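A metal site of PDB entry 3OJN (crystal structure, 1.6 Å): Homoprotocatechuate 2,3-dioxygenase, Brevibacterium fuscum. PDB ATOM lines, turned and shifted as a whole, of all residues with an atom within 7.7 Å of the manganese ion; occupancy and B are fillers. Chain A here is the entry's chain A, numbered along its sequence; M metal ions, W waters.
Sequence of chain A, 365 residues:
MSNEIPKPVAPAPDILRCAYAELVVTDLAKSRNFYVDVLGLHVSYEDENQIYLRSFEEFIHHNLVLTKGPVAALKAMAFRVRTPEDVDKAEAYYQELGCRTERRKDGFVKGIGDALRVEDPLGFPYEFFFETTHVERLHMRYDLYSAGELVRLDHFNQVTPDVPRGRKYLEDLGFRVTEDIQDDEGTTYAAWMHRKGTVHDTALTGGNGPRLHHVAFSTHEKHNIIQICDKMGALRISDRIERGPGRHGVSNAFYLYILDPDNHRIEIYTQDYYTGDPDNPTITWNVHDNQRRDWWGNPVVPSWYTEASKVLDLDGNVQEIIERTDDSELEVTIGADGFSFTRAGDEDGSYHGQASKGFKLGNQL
The side-chain hydroxyl (OH) of Tyr 257 sits at hydrogen-bond distance from the side-chain carboxylate (OE2) of Glu 267, at 3.3 Å. A ring nitrogen (NE2) of His 248 is in hydrogen-bond range of the side-chain carboxylate (OE2) of Glu 267 (2.8 Å). The backbone NH (N) of Glu 267 is in hydrogen-bond range of the backbone carbonyl oxygen (O) of Val 215, 2.9 Å away. The backbone carbonyl oxygen (O) of His 214 sits at hydrogen-bond distance from the backbone NH (N) of Asn 157. A ring nitrogen (ND1) of His 214 lies within hydrogen-bond range of a ring nitrogen (ND1) of His 213, 2.9 Å away. A ring nitrogen (ND1) of His 155 lies close to a ring nitrogen (NE2) of His 200. The backbone carbonyl oxygen (O) of His 155 lies within hydrogen-bond range of the backbone NH (N) of Ala 216 (2.9 Å). The side-chain carboxylate (OD2) of Asp 154 lies within hydrogen-bond range of a ring nitrogen (ND1) of His 155, 2.8 Å away.
NE2 of His 200 touches the manganese ion, at 3.95 Å. Within 4 Å of the manganese ion: His 155, His 200, His 214 and Glu 267. The nearest printed residue that does not touch the manganese ion is Tyr 257 (4.1 Å).
The manganese ion is bound by OE1 of Glu 267 (2.1 Å), NE2 of His 214 (2.2 Å), water W2 (2.2 Å), water W1 (2.2 Å), NE2 of His 155 (2.3 Å) and water W3 (2.5 Å). The manganese ion has six donor atoms within binding distance.
Water W1 bridges NE2 of His 200 (2.8 Å) and ND2 of Asn 157 (2.8 Å).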
ATOM      1  N   ASP A 154      20.320   4.152  27.618  1.00  0.00           N
ATOM      2  CA  ASP A 154      21.146   4.767  26.566  1.00  0.00           C
ATOM      3  C   ASP A 154      21.033   4.128  25.163  1.00  0.00           C
ATOM      4  O   ASP A 154      20.920   4.869  24.157  1.00  0.00           O
ATOM      5  CB  ASP A 154      22.630   4.869  26.936  1.00  0.00           C
ATOM      6  CG  ASP A 154      23.398   5.745  25.925  1.00  0.00           C
ATOM      7  OD1 ASP A 154      23.186   6.991  25.958  1.00  0.00           O
ATOM      8  OD2 ASP A 154      24.120   5.201  25.014  1.00  0.00           O
ATOM      9  N   HIS A 155      21.122   2.816  25.088  1.00  0.00           N
ATOM     10  CA  HIS A 155      21.149   2.119  23.790  1.00  0.00           C
ATOM     11  C   HIS A 155      20.894   0.635  23.880  1.00  0.00           C
ATOM     12  O   HIS A 155      20.926   0.033  24.947  1.00  0.00           O
ATOM     13  CB  HIS A 155      22.505   2.314  23.105  1.00  0.00           C
ATOM     14  CG  HIS A 155      23.678   1.711  23.833  1.00  0.00           C
ATOM     15  ND1 HIS A 155      24.473   2.453  24.653  1.00  0.00           N
ATOM     16  CD2 HIS A 155      24.247   0.480  23.761  1.00  0.00           C
ATOM     17  CE1 HIS A 155      25.470   1.701  25.111  1.00  0.00           C
ATOM     18  NE2 HIS A 155      25.359   0.501  24.585  1.00  0.00           N
ATOM     19  N   PHE A 156      20.677   0.053  22.703  1.00  0.00           N
ATOM     20  CA  PHE A 156      20.619  -1.370  22.511  1.00  0.00           C
ATOM     21  C   PHE A 156      21.840  -1.769  21.670  1.00  0.00           C
ATOM     22  O   PHE A 156      22.449  -0.916  21.001  1.00  0.00           O
ATOM     23  CB  PHE A 156      19.378  -1.739  21.688  1.00  0.00           C
ATOM     24  CG  PHE A 156      18.069  -1.198  22.213  1.00  0.00           C
ATOM     25  CD1 PHE A 156      17.666  -1.429  23.512  1.00  0.00           C
ATOM     26  CD2 PHE A 156      17.211  -0.520  21.364  1.00  0.00           C
ATOM     27  CE1 PHE A 156      16.444  -0.951  23.988  1.00  0.00           C
ATOM     28  CE2 PHE A 156      15.992  -0.023  21.824  1.00  0.00           C
ATOM     29  CZ  PHE A 156      15.608  -0.245  23.117  1.00  0.00           C
ATOM     30  N   ASN A 157      22.201  -3.040  21.718  1.00  0.00           N
ATOM     31  CA  ASN A 157      23.277  -3.557  20.837  1.00  0.00           C
ATOM     32  C   ASN A 157      22.825  -4.926  20.318  1.00  0.00           C
ATOM     33  O   ASN A 157      22.489  -5.813  21.094  1.00  0.00           O
ATOM     34  CB  ASN A 157      24.622  -3.572  21.578  1.00  0.00           C
ATOM     35  CG  ASN A 157      25.785  -3.958  20.685  1.00  0.00           C
ATOM     36  OD1 ASN A 157      25.768  -4.999  20.048  1.00  0.00           O
ATOM     37  ND2 ASN A 157      26.834  -3.106  20.653  1.00  0.00           N
ATOM     38  N   TRP A 192      28.149   1.602  15.104  1.00  0.00           N
ATOM     39  CA  TRP A 192      27.341   2.293  16.085  1.00  0.00           C
ATOM     40  C   TRP A 192      26.567   3.384  15.385  1.00  0.00           C
ATOM     41  O   TRP A 192      27.148   4.129  14.581  1.00  0.00           O
ATOM     42  CB  TRP A 192      28.287   2.935  17.098  1.00  0.00           C
ATOM     43  CG  TRP A 192      28.906   2.012  18.072  1.00  0.00           C
ATOM     44  CD1 TRP A 192      28.627   1.949  19.419  1.00  0.00           C
ATOM     45  CD2 TRP A 192      29.936   1.034  17.849  1.00  0.00           C
ATOM     46  NE1 TRP A 192      29.383   0.994  20.035  1.00  0.00           N
ATOM     47  CE2 TRP A 192      30.209   0.415  19.101  1.00  0.00           C
ATOM     48  CE3 TRP A 192      30.707   0.664  16.742  1.00  0.00           C
ATOM     49  CZ2 TRP A 192      31.156  -0.599  19.261  1.00  0.00           C
ATOM     50  CZ3 TRP A 192      31.646  -0.375  16.889  1.00  0.00           C
ATOM     51  CH2 TRP A 192      31.882  -0.970  18.140  1.00  0.00           C
ATOM     52  N   HIS A 200      25.247   6.444  20.245  1.00  0.00           N
ATOM     53  CA  HIS A 200      24.285   5.547  19.644  1.00  0.00           C
ATOM     54  C   HIS A 200      22.992   5.370  20.387  1.00  0.00           C
ATOM     55  O   HIS A 200      22.905   5.580  21.590  1.00  0.00           O
ATOM     56  CB  HIS A 200      24.887   4.176  19.327  1.00  0.00           C
ATOM     57  CG  HIS A 200      25.465   3.431  20.480  1.00  0.00           C
ATOM     58  ND1 HIS A 200      26.264   4.018  21.449  1.00  0.00           N
ATOM     59  CD2 HIS A 200      25.475   2.097  20.739  1.00  0.00           C
ATOM     60  CE1 HIS A 200      26.709   3.061  22.268  1.00  0.00           C
ATOM     61  NE2 HIS A 200      26.270   1.898  21.843  1.00  0.00           N
ATOM     62  N   ALA A 203      23.367  -0.460  17.969  1.00  0.00           N
ATOM     63  CA  ALA A 203      24.646  -0.825  17.401  1.00  0.00           C
ATOM     64  C   ALA A 203      24.516  -2.224  16.861  1.00  0.00           C
ATOM     65  O   ALA A 203      23.695  -3.017  17.316  1.00  0.00           O
ATOM     66  CB  ALA A 203      25.746  -0.752  18.444  1.00  0.00           C
ATOM     67  N   THR A 205      26.702  -5.648  16.081  1.00  0.00           N
ATOM     68  CA  THR A 205      27.910  -6.405  16.369  1.00  0.00           C
ATOM     69  C   THR A 205      27.827  -7.621  15.483  1.00  0.00           C
ATOM     70  O   THR A 205      26.786  -8.294  15.420  1.00  0.00           O
ATOM     71  CB  THR A 205      27.962  -6.825  17.833  1.00  0.00           C
ATOM     72  OG1 THR A 205      27.957  -5.652  18.658  1.00  0.00           O
ATOM     73  CG2 THR A 205      29.193  -7.696  18.117  1.00  0.00           C
ATOM     74  N   HIS A 213      22.700  -8.412  21.996  1.00  0.00           N
ATOM     75  CA  HIS A 213      23.915  -8.415  22.775  1.00  0.00           C
ATOM     76  C   HIS A 213      23.717  -7.857  24.177  1.00  0.00           C
ATOM     77  O   HIS A 213      24.109  -8.515  25.136  1.00  0.00           O
ATOM     78  CB  HIS A 213      25.055  -7.684  22.077  1.00  0.00           C
ATOM     79  CG  HIS A 213      26.391  -8.102  22.599  1.00  0.00           C
ATOM     80  ND1 HIS A 213      26.917  -7.626  23.774  1.00  0.00           N
ATOM     81  CD2 HIS A 213      27.269  -9.030  22.143  1.00  0.00           C
ATOM     82  CE1 HIS A 213      28.087  -8.195  24.004  1.00  0.00           C
ATOM     83  NE2 HIS A 213      28.320  -9.062  23.038  1.00  0.00           N
ATOM     84  N   HIS A 214      23.196  -6.650  24.285  1.00  0.00           N
ATOM     85  CA  HIS A 214      22.941  -6.039  25.581  1.00  0.00           C
ATOM     86  C   HIS A 214      21.986  -4.845  25.466  1.00  0.00           C
ATOM     87  O   HIS A 214      21.683  -4.368  24.367  1.00  0.00           O
ATOM     88  CB  HIS A 214      24.274  -5.584  26.253  1.00  0.00           C
ATOM     89  CG  HIS A 214      25.081  -4.608  25.449  1.00  0.00           C
ATOM     90  ND1 HIS A 214      26.089  -5.018  24.612  1.00  0.00           N
ATOM     91  CD2 HIS A 214      25.104  -3.258  25.424  1.00  0.00           C
ATOM     92  CE1 HIS A 214      26.673  -3.965  24.072  1.00  0.00           C
ATOM     93  NE2 HIS A 214      26.088  -2.883  24.538  1.00  0.00           N
ATOM     94  N   VAL A 215      21.502  -4.415  26.630  1.00  0.00           N
ATOM     95  CA  VAL A 215      20.785  -3.166  26.786  1.00  0.00           C
ATOM     96  C   VAL A 215      21.665  -2.347  27.737  1.00  0.00           C
ATOM     97  O   VAL A 215      22.227  -2.888  28.701  1.00  0.00           O
ATOM     98  CB  VAL A 215      19.384  -3.387  27.437  1.00  0.00           C
ATOM     99  CG1 VAL A 215      18.729  -2.041  27.726  1.00  0.00           C
ATOM    100  CG2 VAL A 215      18.479  -4.242  26.503  1.00  0.00           C
ATOM    101  N   ALA A 216      21.787  -1.044  27.495  1.00  0.00           N
ATOM    102  CA  ALA A 216      22.684  -0.230  28.289  1.00  0.00           C
ATOM    103  C   ALA A 216      21.945   0.917  28.978  1.00  0.00           C
ATOM    104  O   ALA A 216      21.135   1.625  28.349  1.00  0.00           O
ATOM    105  CB  ALA A 216      23.786   0.352  27.386  1.00  0.00           C
ATOM    106  N   HIS A 248      35.936   2.628  27.145  1.00  0.00           N
ATOM    107  CA  HIS A 248      35.826   2.152  25.767  1.00  0.00           C
ATOM    108  C   HIS A 248      36.764   2.993  24.887  1.00  0.00           C
ATOM    109  O   HIS A 248      36.981   4.185  25.138  1.00  0.00           O
ATOM    110  CB  HIS A 248      34.405   2.313  25.202  1.00  0.00           C
ATOM    111  CG  HIS A 248      33.453   1.252  25.621  1.00  0.00           C
ATOM    112  ND1 HIS A 248      33.731  -0.095  25.467  1.00  0.00           N
ATOM    113  CD2 HIS A 248      32.200   1.328  26.135  1.00  0.00           C
ATOM    114  CE1 HIS A 248      32.701  -0.802  25.897  1.00  0.00           C
ATOM    115  NE2 HIS A 248      31.762   0.037  26.295  1.00  0.00           N
ATOM    116  N   SER A 251      33.386   4.992  21.275  1.00  0.00           N
ATOM    117  CA  SER A 251      32.410   5.694  22.146  1.00  0.00           C
ATOM    118  C   SER A 251      33.041   6.530  23.246  1.00  0.00           C
ATOM    119  O   SER A 251      32.426   7.495  23.684  1.00  0.00           O
ATOM    120  CB  SER A 251      31.334   4.799  22.776  1.00  0.00           C
ATOM    121  OG  SER A 251      31.788   4.125  23.922  1.00  0.00           O
ATOM    122  N   TYR A 255      32.541   2.111  31.248  1.00  0.00           N
ATOM    123  CA  TYR A 255      31.593   1.008  31.105  1.00  0.00           C
ATOM    124  C   TYR A 255      31.780  -0.146  32.056  1.00  0.00           C
ATOM    125  O   TYR A 255      32.853  -0.296  32.673  1.00  0.00           O
ATOM    126  CB  TYR A 255      31.637   0.429  29.687  1.00  0.00           C
ATOM    127  CG  TYR A 255      32.869  -0.408  29.426  1.00  0.00           C
ATOM    128  CD1 TYR A 255      34.024   0.170  28.913  1.00  0.00           C
ATOM    129  CD2 TYR A 255      32.875  -1.776  29.662  1.00  0.00           C
ATOM    130  CE1 TYR A 255      35.159  -0.585  28.651  1.00  0.00           C
ATOM    131  CE2 TYR A 255      34.028  -2.549  29.445  1.00  0.00           C
ATOM    132  CZ  TYR A 255      35.167  -1.938  28.925  1.00  0.00           C
ATOM    133  OH  TYR A 255      36.309  -2.679  28.655  1.00  0.00           O
ATOM    134  N   TYR A 257      29.989  -4.447  32.077  1.00  0.00           N
ATOM    135  CA  TYR A 257      29.019  -5.470  31.626  1.00  0.00           C
ATOM    136  C   TYR A 257      28.770  -6.471  32.754  1.00  0.00           C
ATOM    137  O   TYR A 257      29.725  -7.101  33.277  1.00  0.00           O
ATOM    138  CB  TYR A 257      29.537  -6.227  30.385  1.00  0.00           C
ATOM    139  CG  TYR A 257      29.766  -5.348  29.189  1.00  0.00           C
ATOM    140  CD1 TYR A 257      28.737  -5.011  28.332  1.00  0.00           C
ATOM    141  CD2 TYR A 257      31.024  -4.823  28.924  1.00  0.00           C
ATOM    142  CE1 TYR A 257      28.946  -4.165  27.252  1.00  0.00           C
ATOM    143  CE2 TYR A 257      31.242  -3.979  27.822  1.00  0.00           C
ATOM    144  CZ  TYR A 257      30.212  -3.672  26.999  1.00  0.00           C
ATOM    145  OH  TYR A 257      30.421  -2.862  25.919  1.00  0.00           O
ATOM    146  N   GLU A 267      24.733  -3.435  30.134  1.00  0.00           N
ATOM    147  CA  GLU A 267      25.862  -2.511  30.205  1.00  0.00           C
ATOM    148  C   GLU A 267      25.495  -1.279  31.043  1.00  0.00           C
ATOM    149  O   GLU A 267      24.388  -0.733  30.926  1.00  0.00           O
ATOM    150  CB  GLU A 267      26.289  -2.026  28.816  1.00  0.00           C
ATOM    151  CG  GLU A 267      27.618  -1.270  28.826  1.00  0.00           C
ATOM    152  CD  GLU A 267      28.030  -0.773  27.470  1.00  0.00           C
ATOM    153  OE1 GLU A 267      27.254  -0.986  26.520  1.00  0.00           O
ATOM    154  OE2 GLU A 267      29.135  -0.170  27.337  1.00  0.00           O
ATOM    155  N   ILE A 268      26.434  -0.835  31.879  1.00  0.00           N
ATOM    156  CA  ILE A 268      26.337   0.443  32.547  1.00  0.00           C
ATOM    157  C   ILE A 268      27.384   1.326  31.870  1.00  0.00           C
ATOM    158  O   ILE A 268      28.499   0.860  31.616  1.00  0.00           O
ATOM    159  CB  ILE A 268      26.574   0.350  34.058  1.00  0.00           C
ATOM    160  CG1 ILE A 268      25.973  -0.922  34.681  1.00  0.00           C
ATOM    161  CG2 ILE A 268      26.049   1.623  34.746  1.00  0.00           C
ATOM    162  CD1 ILE A 268      24.512  -1.062  34.566  1.00  0.00           C
ATOM    163  N   TYR A 269      27.034   2.564  31.547  1.00  0.00           N
ATOM    164  CA  TYR A 269      27.731   3.381  30.537  1.00  0.00           C
ATOM    165  C   TYR A 269      27.674   4.859  30.919  1.00  0.00           C
ATOM    166  O   TYR A 269      26.666   5.330  31.447  1.00  0.00           O
ATOM    167  CB  TYR A 269      26.988   3.143  29.217  1.00  0.00           C
ATOM    168  CG  TYR A 269      27.386   3.834  27.950  1.00  0.00           C
ATOM    169  CD1 TYR A 269      28.222   3.208  27.030  1.00  0.00           C
ATOM    170  CD2 TYR A 269      26.859   5.084  27.610  1.00  0.00           C
ATOM    171  CE1 TYR A 269      28.531   3.777  25.827  1.00  0.00           C
ATOM    172  CE2 TYR A 269      27.179   5.697  26.406  1.00  0.00           C
ATOM    173  CZ  TYR A 269      28.012   5.016  25.501  1.00  0.00           C
ATOM    174  OH  TYR A 269      28.336   5.541  24.283  1.00  0.00           O
ATOM    175  N   ARG A 293      38.277  -1.522  22.011  1.00  0.00           N
ATOM    176  CA  ARG A 293      37.136  -1.908  22.820  1.00  0.00           C
ATOM    177  C   ARG A 293      37.362  -1.519  24.283  1.00  0.00           C
ATOM    178  O   ARG A 293      36.489  -0.924  24.890  1.00  0.00           O
ATOM    179  CB  ARG A 293      36.812  -3.386  22.660  1.00  0.00           C
ATOM    180  CG  ARG A 293      36.195  -3.689  21.293  1.00  0.00           C
ATOM    181  CD  ARG A 293      35.425  -4.991  21.292  1.00  0.00           C
ATOM    182  NE  ARG A 293      34.692  -5.190  20.025  1.00  0.00           N
ATOM    183  CZ  ARG A 293      33.490  -4.702  19.725  1.00  0.00           C
ATOM    184  NH1 ARG A 293      32.830  -3.917  20.568  1.00  0.00           N
ATOM    185  NH2 ARG A 293      32.926  -5.020  18.569  1.00  0.00           N
ATOM    186  N   TRP A 304      32.090 -12.586  25.940  1.00  0.00           N
ATOM    187  CA  TRP A 304      31.522 -11.347  25.447  1.00  0.00           C
ATOM    188  C   TRP A 304      31.241 -11.418  23.939  1.00  0.00           C
ATOM    189  O   TRP A 304      30.262 -10.835  23.452  1.00  0.00           O
ATOM    190  CB  TRP A 304      32.454 -10.190  25.786  1.00  0.00           C
ATOM    191  CG  TRP A 304      31.803  -8.856  25.678  1.00  0.00           C
ATOM    192  CD1 TRP A 304      31.123  -8.205  26.671  1.00  0.00           C
ATOM    193  CD2 TRP A 304      31.739  -8.019  24.528  1.00  0.00           C
ATOM    194  NE1 TRP A 304      30.655  -7.014  26.204  1.00  0.00           N
ATOM    195  CE2 TRP A 304      30.986  -6.890  24.885  1.00  0.00           C
ATOM    196  CE3 TRP A 304      32.205  -8.146  23.212  1.00  0.00           C
ATOM    197  CZ2 TRP A 304      30.736  -5.837  23.982  1.00  0.00           C
ATOM    198  CZ3 TRP A 304      31.948  -7.106  22.317  1.00  0.00           C
ATOM    199  CH2 TRP A 304      31.207  -5.977  22.709  1.00  0.00           C
HETATM  200 MN    MN M   1      27.117  -0.969  24.428  1.00  0.00          MN
HETATM  201  O   HOH W   1      27.119  -0.760  22.223  1.00  0.00           O
HETATM  202  O   HOH W   2      28.568   0.665  24.651  1.00  0.00           O
HETATM  203  O   HOH W   3      29.207  -2.153  23.904  1.00  0.00           O
